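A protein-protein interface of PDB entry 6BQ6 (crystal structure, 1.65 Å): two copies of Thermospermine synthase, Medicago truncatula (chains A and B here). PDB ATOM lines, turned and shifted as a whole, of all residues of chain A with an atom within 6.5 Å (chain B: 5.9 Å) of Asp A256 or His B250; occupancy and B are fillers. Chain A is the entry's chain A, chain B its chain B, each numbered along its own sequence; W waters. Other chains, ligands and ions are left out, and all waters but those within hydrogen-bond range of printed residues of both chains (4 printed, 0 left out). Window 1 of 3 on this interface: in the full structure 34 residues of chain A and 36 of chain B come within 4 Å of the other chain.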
ATOM      1  N   ILE A  35       3.909   3.630 -15.653  1.00  0.00           N
ATOM      2  CA  ILE A  35       4.017   2.303 -15.072  1.00  0.00           C
ATOM      3  C   ILE A  35       2.953   2.131 -13.966  1.00  0.00           C
ATOM      4  O   ILE A  35       2.448   1.009 -13.749  1.00  0.00           O
ATOM      5  CB  ILE A  35       5.499   1.917 -14.756  1.00  0.00           C
ATOM      6  CG1 ILE A  35       6.224   2.941 -13.954  1.00  0.00           C
ATOM      7  CG2 ILE A  35       6.278   1.672 -16.049  1.00  0.00           C
ATOM      8  CD1 ILE A  35       7.581   2.459 -13.542  1.00  0.00           C
ATOM      9  N   PRO A 220       4.730  -7.299 -10.040  1.00  0.00           N
ATOM     10  CA  PRO A 220       5.627  -6.481  -9.211  1.00  0.00           C
ATOM     11  C   PRO A 220       5.733  -7.006  -7.822  1.00  0.00           C
ATOM     12  O   PRO A 220       4.755  -7.503  -7.247  1.00  0.00           O
ATOM     13  CB  PRO A 220       4.981  -5.094  -9.267  1.00  0.00           C
ATOM     14  CG  PRO A 220       4.091  -5.084 -10.437  1.00  0.00           C
ATOM     15  CD  PRO A 220       3.608  -6.504 -10.554  1.00  0.00           C
ATOM     16  N   ALA A 221       6.922  -6.914  -7.243  1.00  0.00           N
ATOM     17  CA  ALA A 221       7.172  -7.445  -5.888  1.00  0.00           C
ATOM     18  C   ALA A 221       7.963  -6.462  -5.037  1.00  0.00           C
ATOM     19  O   ALA A 221       8.738  -6.850  -4.172  1.00  0.00           O
ATOM     20  CB  ALA A 221       7.811  -8.810  -5.939  1.00  0.00           C
ATOM     21  N   GLY A 222       7.692  -5.178  -5.288  1.00  0.00           N
ATOM     22  CA  GLY A 222       8.262  -4.058  -4.511  1.00  0.00           C
ATOM     23  C   GLY A 222       7.664  -3.996  -3.119  1.00  0.00           C
ATOM     24  O   GLY A 222       6.613  -4.586  -2.811  1.00  0.00           O
ATOM     25  N   ILE A 223       8.345  -3.253  -2.272  1.00  0.00           N
ATOM     26  CA  ILE A 223       7.914  -3.154  -0.878  1.00  0.00           C
ATOM     27  C   ILE A 223       6.428  -2.732  -0.750  1.00  0.00           C
ATOM     28  O   ILE A 223       5.731  -3.249   0.115  1.00  0.00           O
ATOM     29  CB  ILE A 223       8.857  -2.235  -0.092  1.00  0.00           C
ATOM     30  CG1 ILE A 223       8.396  -2.162   1.391  1.00  0.00           C
ATOM     31  CG2 ILE A 223       8.906  -0.850  -0.717  1.00  0.00           C
ATOM     32  CD1 ILE A 223       9.204  -2.989   2.290  1.00  0.00           C
ATOM     33  N   SER A 225       4.501  -2.229  -4.021  1.00  0.00           N
ATOM     34  CA  SER A 225       3.852  -2.718  -5.227  1.00  0.00           C
ATOM     35  C   SER A 225       3.469  -4.159  -5.163  1.00  0.00           C
ATOM     36  O   SER A 225       2.575  -4.588  -5.927  1.00  0.00           O
ATOM     37  CB  SER A 225       4.721  -2.457  -6.451  1.00  0.00           C
ATOM     38  OG  SER A 225       5.957  -3.127  -6.394  1.00  0.00           O
ATOM     39  N   HIS A 226       4.075  -4.929  -4.264  1.00  0.00           N
ATOM     40  CA  HIS A 226       3.761  -6.344  -4.160  1.00  0.00           C
ATOM     41  C   HIS A 226       2.316  -6.705  -3.793  1.00  0.00           C
ATOM     42  O   HIS A 226       1.896  -7.798  -4.025  1.00  0.00           O
ATOM     43  CB  HIS A 226       4.717  -7.024  -3.180  1.00  0.00           C
ATOM     44  CG  HIS A 226       4.336  -6.847  -1.763  1.00  0.00           C
ATOM     45  ND1 HIS A 226       4.761  -5.792  -0.995  1.00  0.00           N
ATOM     46  CD2 HIS A 226       3.534  -7.603  -0.967  1.00  0.00           C
ATOM     47  CE1 HIS A 226       4.229  -5.894   0.213  1.00  0.00           C
ATOM     48  NE2 HIS A 226       3.501  -6.992   0.252  1.00  0.00           N
ATOM     49  N   GLU A 228      -0.411  -5.624  -5.116  1.00  0.00           N
ATOM     50  CA  GLU A 228      -1.351  -5.510  -6.223  1.00  0.00           C
ATOM     51  C   GLU A 228      -1.740  -6.900  -6.653  1.00  0.00           C
ATOM     52  O   GLU A 228      -2.927  -7.197  -6.785  1.00  0.00           O
ATOM     53  CB  GLU A 228      -0.747  -4.859  -7.450  1.00  0.00           C
ATOM     54  CG  GLU A 228      -0.230  -3.447  -7.405  1.00  0.00           C
ATOM     55  CD  GLU A 228       0.632  -3.215  -8.662  1.00  0.00           C
ATOM     56  OE1 GLU A 228       1.746  -2.648  -8.519  1.00  0.00           O
ATOM     57  OE2 GLU A 228       0.186  -3.691  -9.782  1.00  0.00           O
ATOM     58  N   ALA A 249      13.369 -10.481  -7.706  1.00  0.00           N
ATOM     59  CA  ALA A 249      14.597  -9.910  -8.161  1.00  0.00           C
ATOM     60  C   ALA A 249      14.341  -8.598  -8.906  1.00  0.00           C
ATOM     61  O   ALA A 249      13.338  -8.433  -9.565  1.00  0.00           O
ATOM     62  CB  ALA A 249      15.318 -10.883  -9.078  1.00  0.00           C
ATOM     63  N   HIS A 250      15.312  -7.691  -8.850  1.00  0.00           N
ATOM     64  CA  HIS A 250      15.216  -6.436  -9.578  1.00  0.00           C
ATOM     65  C   HIS A 250      15.434  -6.619 -11.066  1.00  0.00           C
ATOM     66  O   HIS A 250      16.369  -7.275 -11.476  1.00  0.00           O
ATOM     67  CB  HIS A 250      16.260  -5.489  -9.038  1.00  0.00           C
ATOM     68  CG  HIS A 250      16.174  -4.101  -9.595  1.00  0.00           C
ATOM     69  ND1 HIS A 250      17.224  -3.484 -10.223  1.00  0.00           N
ATOM     70  CD2 HIS A 250      15.157  -3.201  -9.625  1.00  0.00           C
ATOM     71  CE1 HIS A 250      16.876  -2.289 -10.617  1.00  0.00           C
ATOM     72  NE2 HIS A 250      15.631  -2.078 -10.259  1.00  0.00           N
ATOM     73  N   ILE A 251      14.548  -6.067 -11.865  1.00  0.00           N
ATOM     74  CA  ILE A 251      14.766  -5.980 -13.322  1.00  0.00           C
ATOM     75  C   ILE A 251      14.769  -4.480 -13.642  1.00  0.00           C
ATOM     76  O   ILE A 251      13.749  -3.823 -13.561  1.00  0.00           O
ATOM     77  CB  ILE A 251      13.703  -6.773 -14.073  1.00  0.00           C
ATOM     78  CG1 ILE A 251      13.854  -8.332 -13.742  1.00  0.00           C
ATOM     79  CG2 ILE A 251      13.891  -6.586 -15.546  1.00  0.00           C
ATOM     80  CD1 ILE A 251      12.544  -8.988 -13.828  1.00  0.00           C
ATOM     81  N   PRO A 252      15.921  -3.909 -13.979  1.00  0.00           N
ATOM     82  CA  PRO A 252      16.020  -2.471 -14.108  1.00  0.00           C
ATOM     83  C   PRO A 252      15.021  -1.863 -15.070  1.00  0.00           C
ATOM     84  O   PRO A 252      14.342  -0.868 -14.719  1.00  0.00           O
ATOM     85  CB  PRO A 252      17.465  -2.274 -14.599  1.00  0.00           C
ATOM     86  CG  PRO A 252      18.203  -3.445 -14.026  1.00  0.00           C
ATOM     87  CD  PRO A 252      17.241  -4.578 -13.984  1.00  0.00           C
ATOM     88  N   SER A 253      14.847  -2.487 -16.238  1.00  0.00           N
ATOM     89  CA  SER A 253      13.919  -1.933 -17.219  1.00  0.00           C
ATOM     90  C   SER A 253      12.467  -1.918 -16.739  1.00  0.00           C
ATOM     91  O   SER A 253      11.664  -1.179 -17.285  1.00  0.00           O
ATOM     92  CB  SER A 253      14.018  -2.679 -18.516  1.00  0.00           C
ATOM     93  OG  SER A 253      13.715  -4.040 -18.434  1.00  0.00           O
ATOM     94  N   TYR A 254      12.124  -2.772 -15.781  1.00  0.00           N
ATOM     95  CA  TYR A 254      10.757  -2.835 -15.235  1.00  0.00           C
ATOM     96  C   TYR A 254      10.495  -1.796 -14.155  1.00  0.00           C
ATOM     97  O   TYR A 254       9.355  -1.695 -13.677  1.00  0.00           O
ATOM     98  CB  TYR A 254      10.459  -4.265 -14.684  1.00  0.00           C
ATOM     99  CG  TYR A 254      10.406  -5.412 -15.666  1.00  0.00           C
ATOM    100  CD1 TYR A 254      10.568  -5.229 -17.055  1.00  0.00           C
ATOM    101  CD2 TYR A 254      10.140  -6.710 -15.232  1.00  0.00           C
ATOM    102  CE1 TYR A 254      10.481  -6.285 -17.944  1.00  0.00           C
ATOM    103  CE2 TYR A 254      10.081  -7.782 -16.115  1.00  0.00           C
ATOM    104  CZ  TYR A 254      10.227  -7.583 -17.464  1.00  0.00           C
ATOM    105  OH  TYR A 254      10.115  -8.647 -18.316  1.00  0.00           O
ATOM    106  N   ALA A 255      11.510  -1.049 -13.737  1.00  0.00           N
ATOM    107  CA  ALA A 255      11.449  -0.067 -12.681  1.00  0.00           C
ATOM    108  C   ALA A 255      10.909  -0.610 -11.368  1.00  0.00           C
ATOM    109  O   ALA A 255      10.301   0.123 -10.581  1.00  0.00           O
ATOM    110  CB  ALA A 255      10.619   1.155 -13.147  1.00  0.00           C
ATOM    111  N   ASP A 256      11.126  -1.906 -11.108  1.00  0.00           N
ATOM    112  CA  ASP A 256      10.669  -2.499  -9.907  1.00  0.00           C
ATOM    113  C   ASP A 256      11.361  -3.855  -9.703  1.00  0.00           C
ATOM    114  O   ASP A 256      12.032  -4.373 -10.606  1.00  0.00           O
ATOM    115  CB  ASP A 256       9.172  -2.702  -9.999  1.00  0.00           C
ATOM    116  CG  ASP A 256       8.468  -2.667  -8.606  1.00  0.00           C
ATOM    117  OD1 ASP A 256       9.154  -2.692  -7.561  1.00  0.00           O
ATOM    118  OD2 ASP A 256       7.226  -2.612  -8.609  1.00  0.00           O
ATOM    119  N   ILE A 257      11.200  -4.345  -8.499  1.00  0.00           N
ATOM    120  CA  ILE A 257      11.447  -5.742  -8.164  1.00  0.00           C
ATOM    121  C   ILE A 257      10.300  -6.500  -8.816  1.00  0.00           C
ATOM    122  O   ILE A 257       9.159  -6.050  -8.760  1.00  0.00           O
ATOM    123  CB  ILE A 257      11.419  -5.930  -6.650  1.00  0.00           C
ATOM    124  CG1 ILE A 257      12.453  -5.062  -5.964  1.00  0.00           C
ATOM    125  CG2 ILE A 257      11.549  -7.401  -6.277  1.00  0.00           C
ATOM    126  CD1 ILE A 257      13.848  -5.267  -6.481  1.00  0.00           C
ATOM    127  N   TRP A 258      10.630  -7.625  -9.422  1.00  0.00           N
ATOM    128  CA  TRP A 258       9.643  -8.529  -9.983  1.00  0.00           C
ATOM    129  C   TRP A 258       9.603  -9.816  -9.174  1.00  0.00           C
ATOM    130  O   TRP A 258      10.579 -10.248  -8.620  1.00  0.00           O
ATOM    131  CB  TRP A 258       9.926  -8.817 -11.471  1.00  0.00           C
ATOM    132  CG  TRP A 258       8.696  -9.014 -12.210  1.00  0.00           C
ATOM    133  CD1 TRP A 258       8.127 -10.199 -12.617  1.00  0.00           C
ATOM    134  CD2 TRP A 258       7.799  -7.980 -12.599  1.00  0.00           C
ATOM    135  NE1 TRP A 258       6.929  -9.939 -13.224  1.00  0.00           N
ATOM    136  CE2 TRP A 258       6.682  -8.590 -13.198  1.00  0.00           C
ATOM    137  CE3 TRP A 258       7.824  -6.593 -12.480  1.00  0.00           C
ATOM    138  CZ2 TRP A 258       5.621  -7.836 -13.715  1.00  0.00           C
ATOM    139  CZ3 TRP A 258       6.776  -5.857 -12.931  1.00  0.00           C
ATOM    140  CH2 TRP A 258       5.673  -6.475 -13.559  1.00  0.00           C
ATOM    141  N   ILE B  86      13.623   2.876   4.444  1.00  0.00           N
ATOM    142  CA  ILE B  86      14.430   1.794   3.934  1.00  0.00           C
ATOM    143  C   ILE B  86      15.917   2.218   3.896  1.00  0.00           C
ATOM    144  O   ILE B  86      16.767   1.468   4.379  1.00  0.00           O
ATOM    145  CB  ILE B  86      13.969   1.347   2.544  1.00  0.00           C
ATOM    146  CG1 ILE B  86      12.498   0.943   2.577  1.00  0.00           C
ATOM    147  CG2 ILE B  86      14.821   0.188   2.011  1.00  0.00           C
ATOM    148  CD1 ILE B  86      11.966   0.575   1.223  1.00  0.00           C
ATOM    149  N   SER B 248      22.849  -4.398  -0.198  1.00  0.00           N
ATOM    150  CA  SER B 248      21.982  -3.570  -1.020  1.00  0.00           C
ATOM    151  C   SER B 248      20.504  -3.836  -0.816  1.00  0.00           C
ATOM    152  O   SER B 248      20.115  -4.882  -0.276  1.00  0.00           O
ATOM    153  CB  SER B 248      22.367  -3.742  -2.497  1.00  0.00           C
ATOM    154  OG  SER B 248      22.109  -5.078  -2.946  1.00  0.00           O
ATOM    155  N   ALA B 249      19.683  -2.910  -1.262  1.00  0.00           N
ATOM    156  CA  ALA B 249      18.229  -3.031  -1.121  1.00  0.00           C
ATOM    157  C   ALA B 249      17.568  -2.095  -2.070  1.00  0.00           C
ATOM    158  O   ALA B 249      18.061  -1.029  -2.340  1.00  0.00           O
ATOM    159  CB  ALA B 249      17.832  -2.686   0.316  1.00  0.00           C
ATOM    160  N   HIS B 250      16.402  -2.490  -2.557  1.00  0.00           N
ATOM    161  CA  HIS B 250      15.635  -1.613  -3.424  1.00  0.00           C
ATOM    162  C   HIS B 250      14.981  -0.462  -2.704  1.00  0.00           C
ATOM    163  O   HIS B 250      14.348  -0.667  -1.663  1.00  0.00           O
ATOM    164  CB  HIS B 250      14.525  -2.460  -4.059  1.00  0.00           C
ATOM    165  CG  HIS B 250      13.710  -1.743  -5.113  1.00  0.00           C
ATOM    166  ND1 HIS B 250      12.353  -1.586  -5.011  1.00  0.00           N
ATOM    167  CD2 HIS B 250      14.069  -1.126  -6.257  1.00  0.00           C
ATOM    168  CE1 HIS B 250      11.906  -0.879  -6.031  1.00  0.00           C
ATOM    169  NE2 HIS B 250      12.935  -0.594  -6.809  1.00  0.00           N
ATOM    170  N   ILE B 251      15.071   0.722  -3.302  1.00  0.00           N
ATOM    171  CA  ILE B 251      14.375   1.895  -2.805  1.00  0.00           C
ATOM    172  C   ILE B 251      13.490   2.440  -3.960  1.00  0.00           C
ATOM    173  O   ILE B 251      13.981   2.942  -4.932  1.00  0.00           O
ATOM    174  CB  ILE B 251      15.351   2.919  -2.265  1.00  0.00           C
ATOM    175  CG1 ILE B 251      16.093   2.305  -1.043  1.00  0.00           C
ATOM    176  CG2 ILE B 251      14.622   4.175  -1.794  1.00  0.00           C
ATOM    177  CD1 ILE B 251      17.362   2.998  -0.771  1.00  0.00           C
ATOM    178  N   PRO B 252      12.188   2.247  -3.867  1.00  0.00           N
ATOM    179  CA  PRO B 252      11.329   2.508  -5.027  1.00  0.00           C
ATOM    180  C   PRO B 252      11.490   3.901  -5.577  1.00  0.00           C
ATOM    181  O   PRO B 252      11.579   4.054  -6.790  1.00  0.00           O
ATOM    182  CB  PRO B 252       9.911   2.279  -4.475  1.00  0.00           C
ATOM    183  CG  PRO B 252      10.096   1.317  -3.391  1.00  0.00           C
ATOM    184  CD  PRO B 252      11.445   1.568  -2.794  1.00  0.00           C
ATOM    185  N   ALA B 255      14.380   4.458  -8.023  1.00  0.00           N
ATOM    186  CA  ALA B 255      14.355   3.638  -9.239  1.00  0.00           C
ATOM    187  C   ALA B 255      15.571   2.743  -9.404  1.00  0.00           C
ATOM    188  O   ALA B 255      16.035   2.516 -10.512  1.00  0.00           O
ATOM    189  CB  ALA B 255      14.148   4.499 -10.518  1.00  0.00           C
ATOM    190  N   ASP B 256      16.133   2.269  -8.281  1.00  0.00           N
ATOM    191  CA  ASP B 256      17.254   1.384  -8.353  1.00  0.00           C
ATOM    192  C   ASP B 256      17.417   0.700  -7.034  1.00  0.00           C
ATOM    193  O   ASP B 256      16.778   1.066  -6.023  1.00  0.00           O
ATOM    194  CB  ASP B 256      18.543   2.149  -8.676  1.00  0.00           C
ATOM    195  CG  ASP B 256      19.563   1.296  -9.471  1.00  0.00           C
ATOM    196  OD1 ASP B 256      19.397   0.049  -9.578  1.00  0.00           O
ATOM    197  OD2 ASP B 256      20.528   1.908  -9.933  1.00  0.00           O
ATOM    198  N   ILE B 257      18.228  -0.329  -7.098  1.00  0.00           N
ATOM    199  CA  ILE B 257      18.795  -0.941  -5.920  1.00  0.00           C
ATOM    200  C   ILE B 257      19.847   0.093  -5.444  1.00  0.00           C
ATOM    201  O   ILE B 257      20.590   0.646  -6.255  1.00  0.00           O
ATOM    202  CB  ILE B 257      19.458  -2.278  -6.255  1.00  0.00           C
ATOM    203  CG1 ILE B 257      18.458  -3.259  -6.855  1.00  0.00           C
ATOM    204  CG2 ILE B 257      20.087  -2.885  -5.034  1.00  0.00           C
ATOM    205  CD1 ILE B 257      17.325  -3.610  -5.933  1.00  0.00           C
ATOM    206  N   TRP B 258      19.905   0.336  -4.156  1.00  0.00           N
ATOM    207  CA  TRP B 258      20.935   1.150  -3.555  1.00  0.00           C
ATOM    208  C   TRP B 258      21.884   0.309  -2.691  1.00  0.00           C
ATOM    209  O   TRP B 258      21.496  -0.738  -2.140  1.00  0.00           O
ATOM    210  CB  TRP B 258      20.274   2.242  -2.683  1.00  0.00           C
ATOM    211  CG  TRP B 258      21.076   3.462  -2.692  1.00  0.00           C
ATOM    212  CD1 TRP B 258      21.969   3.926  -1.728  1.00  0.00           C
ATOM    213  CD2 TRP B 258      21.181   4.357  -3.787  1.00  0.00           C
ATOM    214  NE1 TRP B 258      22.568   5.076  -2.187  1.00  0.00           N
ATOM    215  CE2 TRP B 258      22.134   5.349  -3.445  1.00  0.00           C
ATOM    216  CE3 TRP B 258      20.587   4.412  -5.055  1.00  0.00           C
ATOM    217  CZ2 TRP B 258      22.432   6.407  -4.323  1.00  0.00           C
ATOM    218  CZ3 TRP B 258      20.963   5.438  -5.934  1.00  0.00           C
ATOM    219  CH2 TRP B 258      21.857   6.386  -5.559  1.00  0.00           C
ATOM    220  N   TYR B 289      11.626  -1.987   7.958  1.00  0.00           N
ATOM    221  CA  TYR B 289      12.217  -2.654   6.794  1.00  0.00           C
ATOM    222  C   TYR B 289      13.064  -3.842   7.217  1.00  0.00           C
ATOM    223  O   TYR B 289      12.996  -4.901   6.623  1.00  0.00           O
ATOM    224  CB  TYR B 289      13.095  -1.715   5.949  1.00  0.00           C
ATOM    225  CG  TYR B 289      13.645  -2.443   4.754  1.00  0.00           C
ATOM    226  CD1 TYR B 289      12.835  -2.793   3.704  1.00  0.00           C
ATOM    227  CD2 TYR B 289      14.975  -2.821   4.718  1.00  0.00           C
ATOM    228  CE1 TYR B 289      13.358  -3.509   2.612  1.00  0.00           C
ATOM    229  CE2 TYR B 289      15.477  -3.509   3.669  1.00  0.00           C
ATOM    230  CZ  TYR B 289      14.703  -3.868   2.658  1.00  0.00           C
ATOM    231  OH  TYR B 289      15.276  -4.593   1.636  1.00  0.00           O
HETATM  232  O   HOH W   1      14.783   0.205 -11.872  1.00  0.00           O
HETATM  233  O   HOH W   2      13.567   0.271  -9.566  1.00  0.00           O
HETATM  234  O   HOH W   3      11.681   1.593  -8.398  1.00  0.00           O
HETATM  235  O   HOH W   4      11.098  -2.825  -2.922  1.00  0.00           O
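The backbone NH of Ala A221 lies within hydrogen-bond range of the backbone carbonyl oxygen of Ile A257 (2.8 Å).
The backbone carbonyl oxygen (O) of Ile A223 sits at hydrogen-bond distance from a ring nitrogen (ND1) of His A226 (2.9 Å).
OD2 of Asp A256 is in hydrogen-bond range of OG of Ser A225 (2.6 Å).
The backbone carbonyl oxygen (O) of Asp A256 is in hydrogen-bond range of the backbone NH (N) of Ile A251.
The backbone carbonyl oxygen of Asp B256 lies within hydrogen-bond range of the backbone NH of Ile B251 (3.2 Å).
Ile A223 touches Ile B86 (CG2 to CD1, 3.9 Å).
Ile A223 touches Pro B252.
Tyr B289 touches Ile A223.
Asp B256 touches His A250 (OD1 to CE1, 3.6 Å).
Ile B257 touches His A250.
His B250 touches Asp A256.
CG1 of Ile A257 touches ND1 of His B250, 3.6 Å away.
Ile A257 touches Ile B257.
Of the printed residues of chain B, Ile A223 touches Ile B86, Pro B252 and Tyr B289.
Ser B248 touches none of the printed residues of chain A.
His B250 touches just these residues of chain A: Asp A256 (3.6 Å) and Ile A257 (3.6 Å).
Printed residues of chain A within 4 Å of Pro B252: Ile A223 (3.6 Å).
Of the printed residues of chain A, Asp B256 touches His A250 (3.6 Å).
The nearest residue of chain A that does not touch His B250 is His A250 (4.1 Å).
Hydrophobic or aromatic side chains of chain A that line the printed part of chain B: Ile A223, His A250 and Ile A257.
Of the 11 printed residues of chain B, 6 touch a printed residue of chain A.
Among the printed residues, no Asp or Glu carboxylate lies within 4 Å of a Lys or Arg side-chain nitrogen of the other chain.
His A250 touches Asp B256, and with the chains exchanged Asp A256 touches His B250.
His A250 touches Ile B257, and with the chains exchanged Ile A257 touches His B250.
Ile B257 touches its own counterpart, Ile A257.
8 positions are printed for both chains.
Water W4 bridges ND1 of His B250 (2.7 Å) and N of Ile A223 (2.9 Å).
Water W1 lies within hydrogen-bond range of a ring nitrogen (NE2) of His A250 (2.9 Å), the backbone carbonyl oxygen (O) of Ala B255 (3.0 Å) and the backbone carbonyl oxygen (O) of Pro A252 (3.1 Å).
Water W3 lies within hydrogen-bond range of the backbone carbonyl oxygen of Pro B252 (2.9 Å), the backbone carbonyl oxygen of Ala A255 (3.0 Å) and a ring nitrogen (NE2) of His B250 (3.0 Å).
Water W2 lies within hydrogen-bond range of a ring nitrogen (NE2) of His B250 (3.0 Å), a ring nitrogen (NE2) of His A250 (3.2 Å), the backbone carbonyl oxygen of Ala A255 (3.4 Å), the backbone carbonyl oxygen of Ala B255 (3.5 Å) and the backbone NH of Asp B256 (3.5 Å).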
